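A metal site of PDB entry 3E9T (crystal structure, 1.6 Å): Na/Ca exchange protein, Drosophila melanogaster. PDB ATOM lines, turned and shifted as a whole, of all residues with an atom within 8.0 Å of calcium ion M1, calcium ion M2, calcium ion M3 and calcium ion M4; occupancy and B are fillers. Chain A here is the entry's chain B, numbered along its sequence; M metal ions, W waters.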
ATOM      1  N   MET A  15      -6.884  -6.832 -20.375  1.00  0.00           N
ATOM      2  CA  MET A  15      -6.646  -6.245 -21.667  1.00  0.00           C
ATOM      3  C   MET A  15      -5.148  -6.235 -21.957  1.00  0.00           C
ATOM      4  O   MET A  15      -4.339  -6.035 -21.036  1.00  0.00           O
ATOM      5  CB  MET A  15      -7.174  -4.803 -21.687  1.00  0.00           C
ATOM      6  CG  MET A  15      -8.666  -4.653 -21.440  1.00  0.00           C
ATOM      7  SD  MET A  15      -9.693  -5.779 -22.391  1.00  0.00           S
ATOM      8  CE  MET A  15      -9.541  -5.151 -24.050  1.00  0.00           C
ATOM      9  N   GLU A  16      -4.785  -6.398 -23.218  1.00  0.00           N
ATOM     10  CA  GLU A  16      -3.376  -6.391 -23.616  1.00  0.00           C
ATOM     11  C   GLU A  16      -2.653  -5.107 -23.217  1.00  0.00           C
ATOM     12  O   GLU A  16      -1.458  -5.137 -22.968  1.00  0.00           O
ATOM     13  CB  GLU A  16      -3.234  -6.614 -25.114  1.00  0.00           C
ATOM     14  CG  GLU A  16      -1.781  -6.807 -25.492  1.00  0.00           C
ATOM     15  CD  GLU A  16      -1.579  -6.954 -26.979  1.00  0.00           C
ATOM     16  OE1 GLU A  16      -0.921  -7.935 -27.384  1.00  0.00           O
ATOM     17  OE2 GLU A  16      -2.065  -6.095 -27.730  1.00  0.00           O
ATOM     18  N   ASN A  17      -3.379  -3.987 -23.158  1.00  0.00           N
ATOM     19  CA  ASN A  17      -2.784  -2.702 -22.790  1.00  0.00           C
ATOM     20  C   ASN A  17      -2.917  -2.321 -21.306  1.00  0.00           C
ATOM     21  O   ASN A  17      -2.794  -1.145 -20.955  1.00  0.00           O
ATOM     22  CB  ASN A  17      -3.332  -1.584 -23.684  1.00  0.00           C
ATOM     23  CG  ASN A  17      -4.836  -1.399 -23.543  1.00  0.00           C
ATOM     24  OD1 ASN A  17      -5.534  -2.263 -22.989  1.00  0.00           O
ATOM     25  ND2 ASN A  17      -5.336  -0.277 -24.025  1.00  0.00           N
ATOM     26  N   CYS A  18      -3.143  -3.316 -20.433  1.00  0.00           N
ATOM     27  CA  CYS A  18      -3.335  -3.066 -19.001  1.00  0.00           C
ATOM     28  C   CYS A  18      -2.034  -2.674 -18.276  1.00  0.00           C
ATOM     29  O   CYS A  18      -2.079  -2.117 -17.171  1.00  0.00           O
ATOM     30  CB  CYS A  18      -3.953  -4.290 -18.311  1.00  0.00           C
ATOM     31  SG  CYS A  18      -2.858  -5.688 -18.089  1.00  0.00           S
ATOM     32  N   THR A  45      -1.729 -20.544 -24.875  1.00  0.00           N
ATOM     33  CA  THR A  45      -1.676 -19.950 -26.218  1.00  0.00           C
ATOM     34  C   THR A  45      -0.985 -18.586 -26.191  1.00  0.00           C
ATOM     35  O   THR A  45      -0.483 -18.123 -27.221  1.00  0.00           O
ATOM     36  CB  THR A  45      -3.073 -19.852 -26.870  1.00  0.00           C
ATOM     37  OG1 THR A  45      -4.007 -19.302 -25.936  1.00  0.00           O
ATOM     38  CG2 THR A  45      -3.539 -21.238 -27.294  1.00  0.00           C
ATOM     39  N   ALA A  46      -0.962 -17.946 -25.018  1.00  0.00           N
ATOM     40  CA  ALA A  46      -0.137 -16.754 -24.793  1.00  0.00           C
ATOM     41  C   ALA A  46       1.238 -17.176 -24.248  1.00  0.00           C
ATOM     42  O   ALA A  46       1.338 -18.134 -23.466  1.00  0.00           O
ATOM     43  CB  ALA A  46      -0.827 -15.814 -23.827  1.00  0.00           C
ATOM     44  N   SER A  47       2.284 -16.464 -24.652  1.00  0.00           N
ATOM     45  CA  SER A  47       3.656 -16.913 -24.393  1.00  0.00           C
ATOM     46  C   SER A  47       4.510 -15.882 -23.679  1.00  0.00           C
ATOM     47  O   SER A  47       4.455 -14.699 -24.021  1.00  0.00           O
ATOM     48  CB  SER A  47       4.328 -17.274 -25.713  1.00  0.00           C
ATOM     49  OG  SER A  47       3.583 -18.267 -26.387  1.00  0.00           O
ATOM     50  N   THR A  50       6.438 -12.706 -25.354  1.00  0.00           N
ATOM     51  CA  THR A  50       5.681 -12.096 -26.441  1.00  0.00           C
ATOM     52  C   THR A  50       4.375 -11.457 -25.929  1.00  0.00           C
ATOM     53  O   THR A  50       4.034 -10.349 -26.322  1.00  0.00           O
ATOM     54  CB  THR A  50       5.410 -13.069 -27.634  1.00  0.00           C
ATOM     55  OG1 THR A  50       4.498 -14.078 -27.244  1.00  0.00           O
ATOM     56  CG2 THR A  50       6.676 -13.761 -28.098  1.00  0.00           C
ATOM     57  N   ASP A  51       3.681 -12.145 -25.023  1.00  0.00           N
ATOM     58  CA  ASP A  51       2.374 -11.700 -24.515  1.00  0.00           C
ATOM     59  C   ASP A  51       2.381 -11.229 -23.074  1.00  0.00           C
ATOM     60  O   ASP A  51       1.539 -10.425 -22.659  1.00  0.00           O
ATOM     61  CB  ASP A  51       1.339 -12.818 -24.668  1.00  0.00           C
ATOM     62  CG  ASP A  51       1.184 -13.249 -26.094  1.00  0.00           C
ATOM     63  OD1 ASP A  51       1.548 -14.396 -26.406  1.00  0.00           O
ATOM     64  OD2 ASP A  51       0.744 -12.401 -26.899  1.00  0.00           O
ATOM     65  N   PHE A  52       3.323 -11.746 -22.293  1.00  0.00           N
ATOM     66  CA  PHE A  52       3.441 -11.336 -20.898  1.00  0.00           C
ATOM     67  C   PHE A  52       4.883 -11.554 -20.505  1.00  0.00           C
ATOM     68  O   PHE A  52       5.595 -12.260 -21.188  1.00  0.00           O
ATOM     69  CB  PHE A  52       2.512 -12.143 -19.983  1.00  0.00           C
ATOM     70  CG  PHE A  52       2.794 -13.655 -19.972  1.00  0.00           C
ATOM     71  CD1 PHE A  52       2.200 -14.504 -20.920  1.00  0.00           C
ATOM     72  CD2 PHE A  52       3.632 -14.212 -19.023  1.00  0.00           C
ATOM     73  CE1 PHE A  52       2.461 -15.888 -20.932  1.00  0.00           C
ATOM     74  CE2 PHE A  52       3.889 -15.599 -19.021  1.00  0.00           C
ATOM     75  CZ  PHE A  52       3.279 -16.426 -19.966  1.00  0.00           C
ATOM     76  N   VAL A  74       1.978  -7.411 -18.602  1.00  0.00           N
ATOM     77  CA  VAL A  74       1.396  -7.850 -19.869  1.00  0.00           C
ATOM     78  C   VAL A  74       2.043  -7.013 -20.989  1.00  0.00           C
ATOM     79  O   VAL A  74       2.256  -5.794 -20.831  1.00  0.00           O
ATOM     80  CB  VAL A  74      -0.148  -7.703 -19.836  1.00  0.00           C
ATOM     81  CG1 VAL A  74      -0.764  -8.064 -21.192  1.00  0.00           C
ATOM     82  CG2 VAL A  74      -0.754  -8.614 -18.730  1.00  0.00           C
ATOM     83  N   ILE A  75       2.428  -7.698 -22.068  1.00  0.00           N
ATOM     84  CA  ILE A  75       3.143  -7.050 -23.182  1.00  0.00           C
ATOM     85  C   ILE A  75       2.163  -6.535 -24.233  1.00  0.00           C
ATOM     86  O   ILE A  75       1.371  -7.282 -24.790  1.00  0.00           O
ATOM     87  CB  ILE A  75       4.240  -7.969 -23.817  1.00  0.00           C
ATOM     88  CG1 ILE A  75       5.288  -8.356 -22.759  1.00  0.00           C
ATOM     89  CG2 ILE A  75       4.896  -7.266 -25.042  1.00  0.00           C
ATOM     90  CD1 ILE A  75       6.333  -9.362 -23.245  1.00  0.00           C
ATOM     91  N   ASP A  76       2.229  -5.226 -24.488  1.00  0.00           N
ATOM     92  CA  ASP A  76       1.362  -4.607 -25.461  1.00  0.00           C
ATOM     93  C   ASP A  76       2.069  -4.570 -26.806  1.00  0.00           C
ATOM     94  O   ASP A  76       3.261  -4.306 -26.873  1.00  0.00           O
ATOM     95  CB  ASP A  76       1.008  -3.174 -25.019  1.00  0.00           C
ATOM     96  CG  ASP A  76      -0.182  -2.596 -25.764  1.00  0.00           C
ATOM     97  OD1 ASP A  76      -0.417  -1.381 -25.627  1.00  0.00           O
ATOM     98  OD2 ASP A  76      -0.889  -3.346 -26.470  1.00  0.00           O
ATOM     99  N   ASP A  77       1.340  -4.848 -27.871  1.00  0.00           N
ATOM    100  CA  ASP A  77       1.863  -4.548 -29.212  1.00  0.00           C
ATOM    101  C   ASP A  77       0.802  -3.907 -30.103  1.00  0.00           C
ATOM    102  O   ASP A  77      -0.277  -3.529 -29.631  1.00  0.00           O
ATOM    103  CB  ASP A  77       2.546  -5.763 -29.867  1.00  0.00           C
ATOM    104  CG  ASP A  77       1.641  -6.968 -29.985  1.00  0.00           C
ATOM    105  OD1 ASP A  77       2.152  -8.099 -29.842  1.00  0.00           O
ATOM    106  OD2 ASP A  77       0.431  -6.800 -30.230  1.00  0.00           O
ATOM    107  N   ASP A  78       1.128  -3.741 -31.385  1.00  0.00           N
ATOM    108  CA  ASP A  78       0.217  -3.115 -32.328  1.00  0.00           C
ATOM    109  C   ASP A  78      -0.386  -4.158 -33.260  1.00  0.00           C
ATOM    110  O   ASP A  78      -1.085  -3.824 -34.226  1.00  0.00           O
ATOM    111  CB  ASP A  78       0.970  -2.053 -33.162  1.00  0.00           C
ATOM    112  CG  ASP A  78       1.331  -0.805 -32.351  1.00  0.00           C
ATOM    113  OD1 ASP A  78       1.104  -0.778 -31.110  1.00  0.00           O
ATOM    114  OD2 ASP A  78       1.846   0.164 -32.961  1.00  0.00           O
ATOM    115  N   VAL A  79      -0.112  -5.431 -32.962  1.00  0.00           N
ATOM    116  CA  VAL A  79      -0.570  -6.547 -33.776  1.00  0.00           C
ATOM    117  C   VAL A  79      -1.887  -7.093 -33.215  1.00  0.00           C
ATOM    118  O   VAL A  79      -1.984  -7.438 -32.036  1.00  0.00           O
ATOM    119  CB  VAL A  79       0.487  -7.689 -33.799  1.00  0.00           C
ATOM    120  CG1 VAL A  79       0.046  -8.820 -34.712  1.00  0.00           C
ATOM    121  CG2 VAL A  79       1.857  -7.148 -34.249  1.00  0.00           C
ATOM    122  N   PHE A  80      -2.902  -7.170 -34.084  1.00  0.00           N
ATOM    123  CA  PHE A  80      -4.161  -7.817 -33.726  1.00  0.00           C
ATOM    124  C   PHE A  80      -3.926  -9.292 -33.392  1.00  0.00           C
ATOM    125  O   PHE A  80      -3.194  -9.987 -34.104  1.00  0.00           O
ATOM    126  CB  PHE A  80      -5.167  -7.701 -34.881  1.00  0.00           C
ATOM    127  CG  PHE A  80      -6.190  -8.796 -34.900  1.00  0.00           C
ATOM    128  CD1 PHE A  80      -6.070  -9.861 -35.790  1.00  0.00           C
ATOM    129  CD2 PHE A  80      -7.254  -8.792 -33.998  1.00  0.00           C
ATOM    130  CE1 PHE A  80      -7.009 -10.896 -35.798  1.00  0.00           C
ATOM    131  CE2 PHE A  80      -8.198  -9.824 -33.999  1.00  0.00           C
ATOM    132  CZ  PHE A  80      -8.070 -10.872 -34.904  1.00  0.00           C
ATOM    133  N   GLU A  81      -4.528  -9.733 -32.287  1.00  0.00           N
ATOM    134  CA  GLU A  81      -4.518 -11.160 -31.893  1.00  0.00           C
ATOM    135  C   GLU A  81      -5.887 -11.614 -31.375  1.00  0.00           C
ATOM    136  O   GLU A  81      -6.659 -10.810 -30.866  1.00  0.00           O
ATOM    137  CB  GLU A  81      -3.486 -11.434 -30.793  1.00  0.00           C
ATOM    138  CG  GLU A  81      -2.055 -11.058 -31.145  1.00  0.00           C
ATOM    139  CD  GLU A  81      -1.275 -10.699 -29.917  1.00  0.00           C
ATOM    140  OE1 GLU A  81      -1.094  -9.484 -29.661  1.00  0.00           O
ATOM    141  OE2 GLU A  81      -0.871 -11.625 -29.171  1.00  0.00           O
ATOM    142  N   GLU A  82      -6.156 -12.909 -31.473  1.00  0.00           N
ATOM    143  CA  GLU A  82      -7.342 -13.497 -30.886  1.00  0.00           C
ATOM    144  C   GLU A  82      -7.180 -13.587 -29.357  1.00  0.00           C
ATOM    145  O   GLU A  82      -6.076 -13.346 -28.848  1.00  0.00           O
ATOM    146  CB  GLU A  82      -7.569 -14.872 -31.507  1.00  0.00           C
ATOM    147  CG  GLU A  82      -7.562 -14.799 -33.045  1.00  0.00           C
ATOM    148  CD  GLU A  82      -7.905 -16.106 -33.733  1.00  0.00           C
ATOM    149  OE1 GLU A  82      -7.986 -16.108 -34.980  1.00  0.00           O
ATOM    150  OE2 GLU A  82      -8.081 -17.142 -33.045  1.00  0.00           O
ATOM    151  N   ASP A  83      -8.247 -13.909 -28.627  1.00  0.00           N
ATOM    152  CA  ASP A  83      -8.117 -14.090 -27.176  1.00  0.00           C
ATOM    153  C   ASP A  83      -7.130 -15.229 -26.917  1.00  0.00           C
ATOM    154  O   ASP A  83      -7.221 -16.276 -27.546  1.00  0.00           O
ATOM    155  CB  ASP A  83      -9.438 -14.455 -26.501  1.00  0.00           C
ATOM    156  CG  ASP A  83     -10.490 -13.363 -26.639  1.00  0.00           C
ATOM    157  OD1 ASP A  83     -10.166 -12.272 -27.172  1.00  0.00           O
ATOM    158  OD2 ASP A  83     -11.665 -13.597 -26.237  1.00  0.00           O
ATOM    159  N   GLU A  84      -6.201 -15.023 -25.987  1.00  0.00           N
ATOM    160  CA  GLU A  84      -5.196 -16.054 -25.671  1.00  0.00           C
ATOM    161  C   GLU A  84      -5.056 -16.208 -24.170  1.00  0.00           C
ATOM    162  O   GLU A  84      -5.294 -15.265 -23.435  1.00  0.00           O
ATOM    163  CB  GLU A  84      -3.846 -15.722 -26.281  1.00  0.00           C
ATOM    164  CG  GLU A  84      -3.874 -15.686 -27.802  1.00  0.00           C
ATOM    165  CD  GLU A  84      -2.523 -15.403 -28.428  1.00  0.00           C
ATOM    166  OE1 GLU A  84      -1.675 -14.744 -27.787  1.00  0.00           O
ATOM    167  OE2 GLU A  84      -2.329 -15.836 -29.584  1.00  0.00           O
ATOM    168  N   ILE A 109      -5.990 -12.982 -21.985  1.00  0.00           N
ATOM    169  CA  ILE A 109      -5.596 -11.681 -22.467  1.00  0.00           C
ATOM    170  C   ILE A 109      -6.490 -11.354 -23.661  1.00  0.00           C
ATOM    171  O   ILE A 109      -6.572 -12.131 -24.626  1.00  0.00           O
ATOM    172  CB  ILE A 109      -4.106 -11.631 -22.931  1.00  0.00           C
ATOM    173  CG1 ILE A 109      -3.133 -11.986 -21.811  1.00  0.00           C
ATOM    174  CG2 ILE A 109      -3.772 -10.210 -23.503  1.00  0.00           C
ATOM    175  CD1 ILE A 109      -1.699 -12.252 -22.319  1.00  0.00           C
ATOM    176  N   LEU A 110      -7.153 -10.211 -23.578  1.00  0.00           N
ATOM    177  CA  LEU A 110      -7.981  -9.703 -24.671  1.00  0.00           C
ATOM    178  C   LEU A 110      -7.220  -8.624 -25.412  1.00  0.00           C
ATOM    179  O   LEU A 110      -6.654  -7.735 -24.787  1.00  0.00           O
ATOM    180  CB  LEU A 110      -9.290  -9.114 -24.138  1.00  0.00           C
ATOM    181  CG  LEU A 110     -10.071  -9.976 -23.136  1.00  0.00           C
ATOM    182  CD1 LEU A 110     -11.327  -9.242 -22.725  1.00  0.00           C
ATOM    183  CD2 LEU A 110     -10.390 -11.371 -23.725  1.00  0.00           C
ATOM    184  N   ASP A 111      -7.192  -8.720 -26.734  1.00  0.00           N
ATOM    185  CA  ASP A 111      -6.441  -7.790 -27.575  1.00  0.00           C
ATOM    186  C   ASP A 111      -7.182  -6.460 -27.693  1.00  0.00           C
ATOM    187  O   ASP A 111      -8.413  -6.415 -27.586  1.00  0.00           O
ATOM    188  CB  ASP A 111      -6.214  -8.410 -28.955  1.00  0.00           C
ATOM    189  CG  ASP A 111      -5.038  -7.803 -29.707  1.00  0.00           C
ATOM    190  OD1 ASP A 111      -3.873  -8.145 -29.402  1.00  0.00           O
ATOM    191  OD2 ASP A 111      -5.277  -7.020 -30.637  1.00  0.00           O
ATOM    192  N   ASP A 112      -6.436  -5.383 -27.933  1.00  0.00           N
ATOM    193  CA  ASP A 112      -7.005  -4.037 -28.088  1.00  0.00           C
ATOM    194  C   ASP A 112      -6.760  -3.429 -29.478  1.00  0.00           C
ATOM    195  O   ASP A 112      -7.205  -2.316 -29.765  1.00  0.00           O
ATOM    196  CB  ASP A 112      -6.442  -3.100 -27.002  1.00  0.00           C
ATOM    197  CG  ASP A 112      -4.927  -2.930 -27.112  1.00  0.00           C
ATOM    198  OD1 ASP A 112      -4.206  -3.928 -27.354  1.00  0.00           O
ATOM    199  OD2 ASP A 112      -4.432  -1.790 -26.956  1.00  0.00           O
ATOM    200  N   ASP A 113      -6.064  -4.179 -30.340  1.00  0.00           N
ATOM    201  CA  ASP A 113      -5.598  -3.681 -31.643  1.00  0.00           C
ATOM    202  C   ASP A 113      -6.605  -3.894 -32.779  1.00  0.00           C
ATOM    203  O   ASP A 113      -6.820  -5.020 -33.251  1.00  0.00           O
ATOM    204  CB  ASP A 113      -4.241  -4.317 -31.996  1.00  0.00           C
ATOM    205  CG  ASP A 113      -3.232  -4.182 -30.863  1.00  0.00           C
ATOM    206  OD1 ASP A 113      -3.070  -3.037 -30.359  1.00  0.00           O
ATOM    207  OD2 ASP A 113      -2.600  -5.186 -30.470  1.00  0.00           O
HETATM  208 CA    CA M   1      -0.749 -10.281 -27.106  1.00  0.00          CA
HETATM  209 CA    CA M   2       0.377 -13.774 -28.950  1.00  0.00          CA
HETATM  210 CA    CA M   3      -2.046  -3.540 -28.296  1.00  0.00          CA
HETATM  211 CA    CA M   4      -1.852  -7.075 -29.894  1.00  0.00          CA
HETATM  212  O   HOH W   1       0.883 -15.760 -28.759  1.00  0.00           O
HETATM  213  O   HOH W   2      -0.233  -9.517 -24.588  1.00  0.00           O
HETATM  214  O   HOH W   3      -3.475  -9.572 -27.293  1.00  0.00           O
HETATM  215  O   HOH W   4      -2.194 -12.307 -26.165  1.00  0.00           O
HETATM  216  O   HOH W   5       1.384  -9.590 -27.753  1.00  0.00           O
HETATM  217  O   HOH W   6       0.364 -13.861 -31.291  1.00  0.00           O
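Of the 26 residues printed, 5 come within 4 Å of calcium ion M3.
The side-chain carboxylate (OD2) of Asp 113 binds calcium ion M4 (2.1 Å).
Calcium ion M4 is bound by the backbone carbonyl oxygen (O) of Val 79.
Calcium ion M4 is bound by OD2 of Asp 77 (2.3 Å).
OD1 of Asp 111 is bound to calcium ion M4 (2.3 Å).
OE2 of Glu 16 binds calcium ion M4 (2.4 Å).
Calcium ion M4 is bound by the side-chain carboxylate (OE1) of Glu 81 (2.5 Å).
OE1 of Glu 16 is bound to calcium ion M4 (2.8 Å).
Calcium ion M4 has seven donor atoms within binding distance.
The backbone NH (N) of Glu 16 sits at hydrogen-bond distance from the backbone carbonyl oxygen (O) of Leu 110, 2.8 Å away.
The side-chain carboxylate (OD2) of Asp 112 sits at hydrogen-bond distance from the side-chain amide nitrogen (ND2) of Asn 17, at 3.4 Å.
The backbone NH (N) of Ile 75 sits at hydrogen-bond distance from the backbone carbonyl oxygen (O) of Asp 51 (2.9 Å).
OD1 of Asp 51 sits close to OG1 of Thr 50, 3.1 Å away.
The backbone NH (N) of Ser 47 lies close to the side-chain carboxylate (OD1) of Asp 51 (2.8 Å).
The backbone NH of Ile 109 is in hydrogen-bond range of the backbone carbonyl oxygen of Glu 84.
Water W2 lies within hydrogen-bond range of O of Ile 75 and O of Asp 51.
Water W5 bridges OD1 of Asp 77 and O of Thr 50.
Water W1 bridges the backbone carbonyl oxygen (O) of Thr 45 and the side-chain carboxylate (OE2) of Glu 84.
Calcium ion M3 is bound by OD2 of Asp 76 (2.2 Å), O of Asp 77 (2.2 Å), OD1 of Asp 113 (2.4 Å), OD1 of Asp 112 (2.4 Å), OE2 of Glu 16 (2.6 Å) and OD2 of Asp 113 (2.8 Å).
Calcium ion M2 is bound by water W1 (2.1 Å), water W6 (2.3 Å), the side-chain carboxylate (OD2) of Asp 51 (2.5 Å), the side-chain carboxylate (OE2) of Glu 81 (2.5 Å), the side-chain carboxylate (OE1) of Glu 84 (2.6 Å) and the side-chain carboxylate (OD1) of Asp 51 (2.9 Å).
Calcium ion M1 is bound by water W5.
The side-chain carboxylate (OE1) of Glu 16 is bound to calcium ion M1, 2.4 Å away.
Calcium ion M1 is bound by OE2 of Glu 81, 2.5 Å away.
Calcium ion M1 is bound by OD2 of Asp 51 (2.6 Å).
Calcium ion M1 is bound by water W4 (2.7 Å).
Water W2 is bound to calcium ion M1, 2.7 Å away.
OE1 of Glu 81 binds calcium ion M1.
Water W3 binds calcium ion M1 (2.8 Å).
Calcium ion M1 has eight donor atoms within binding distance.
Of the 26 residues printed, 6 come within 4 Å of calcium ion M4.
The nearest printed residue that does not touch calcium ion M4 is Phe 80 (4.3 Å).
Within 4 Å of calcium ion M1: Glu 16, Asp 51 and Glu 81.
Along chain A the residues within 4 Å of calcium ion M1 span positions 16 to 81.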
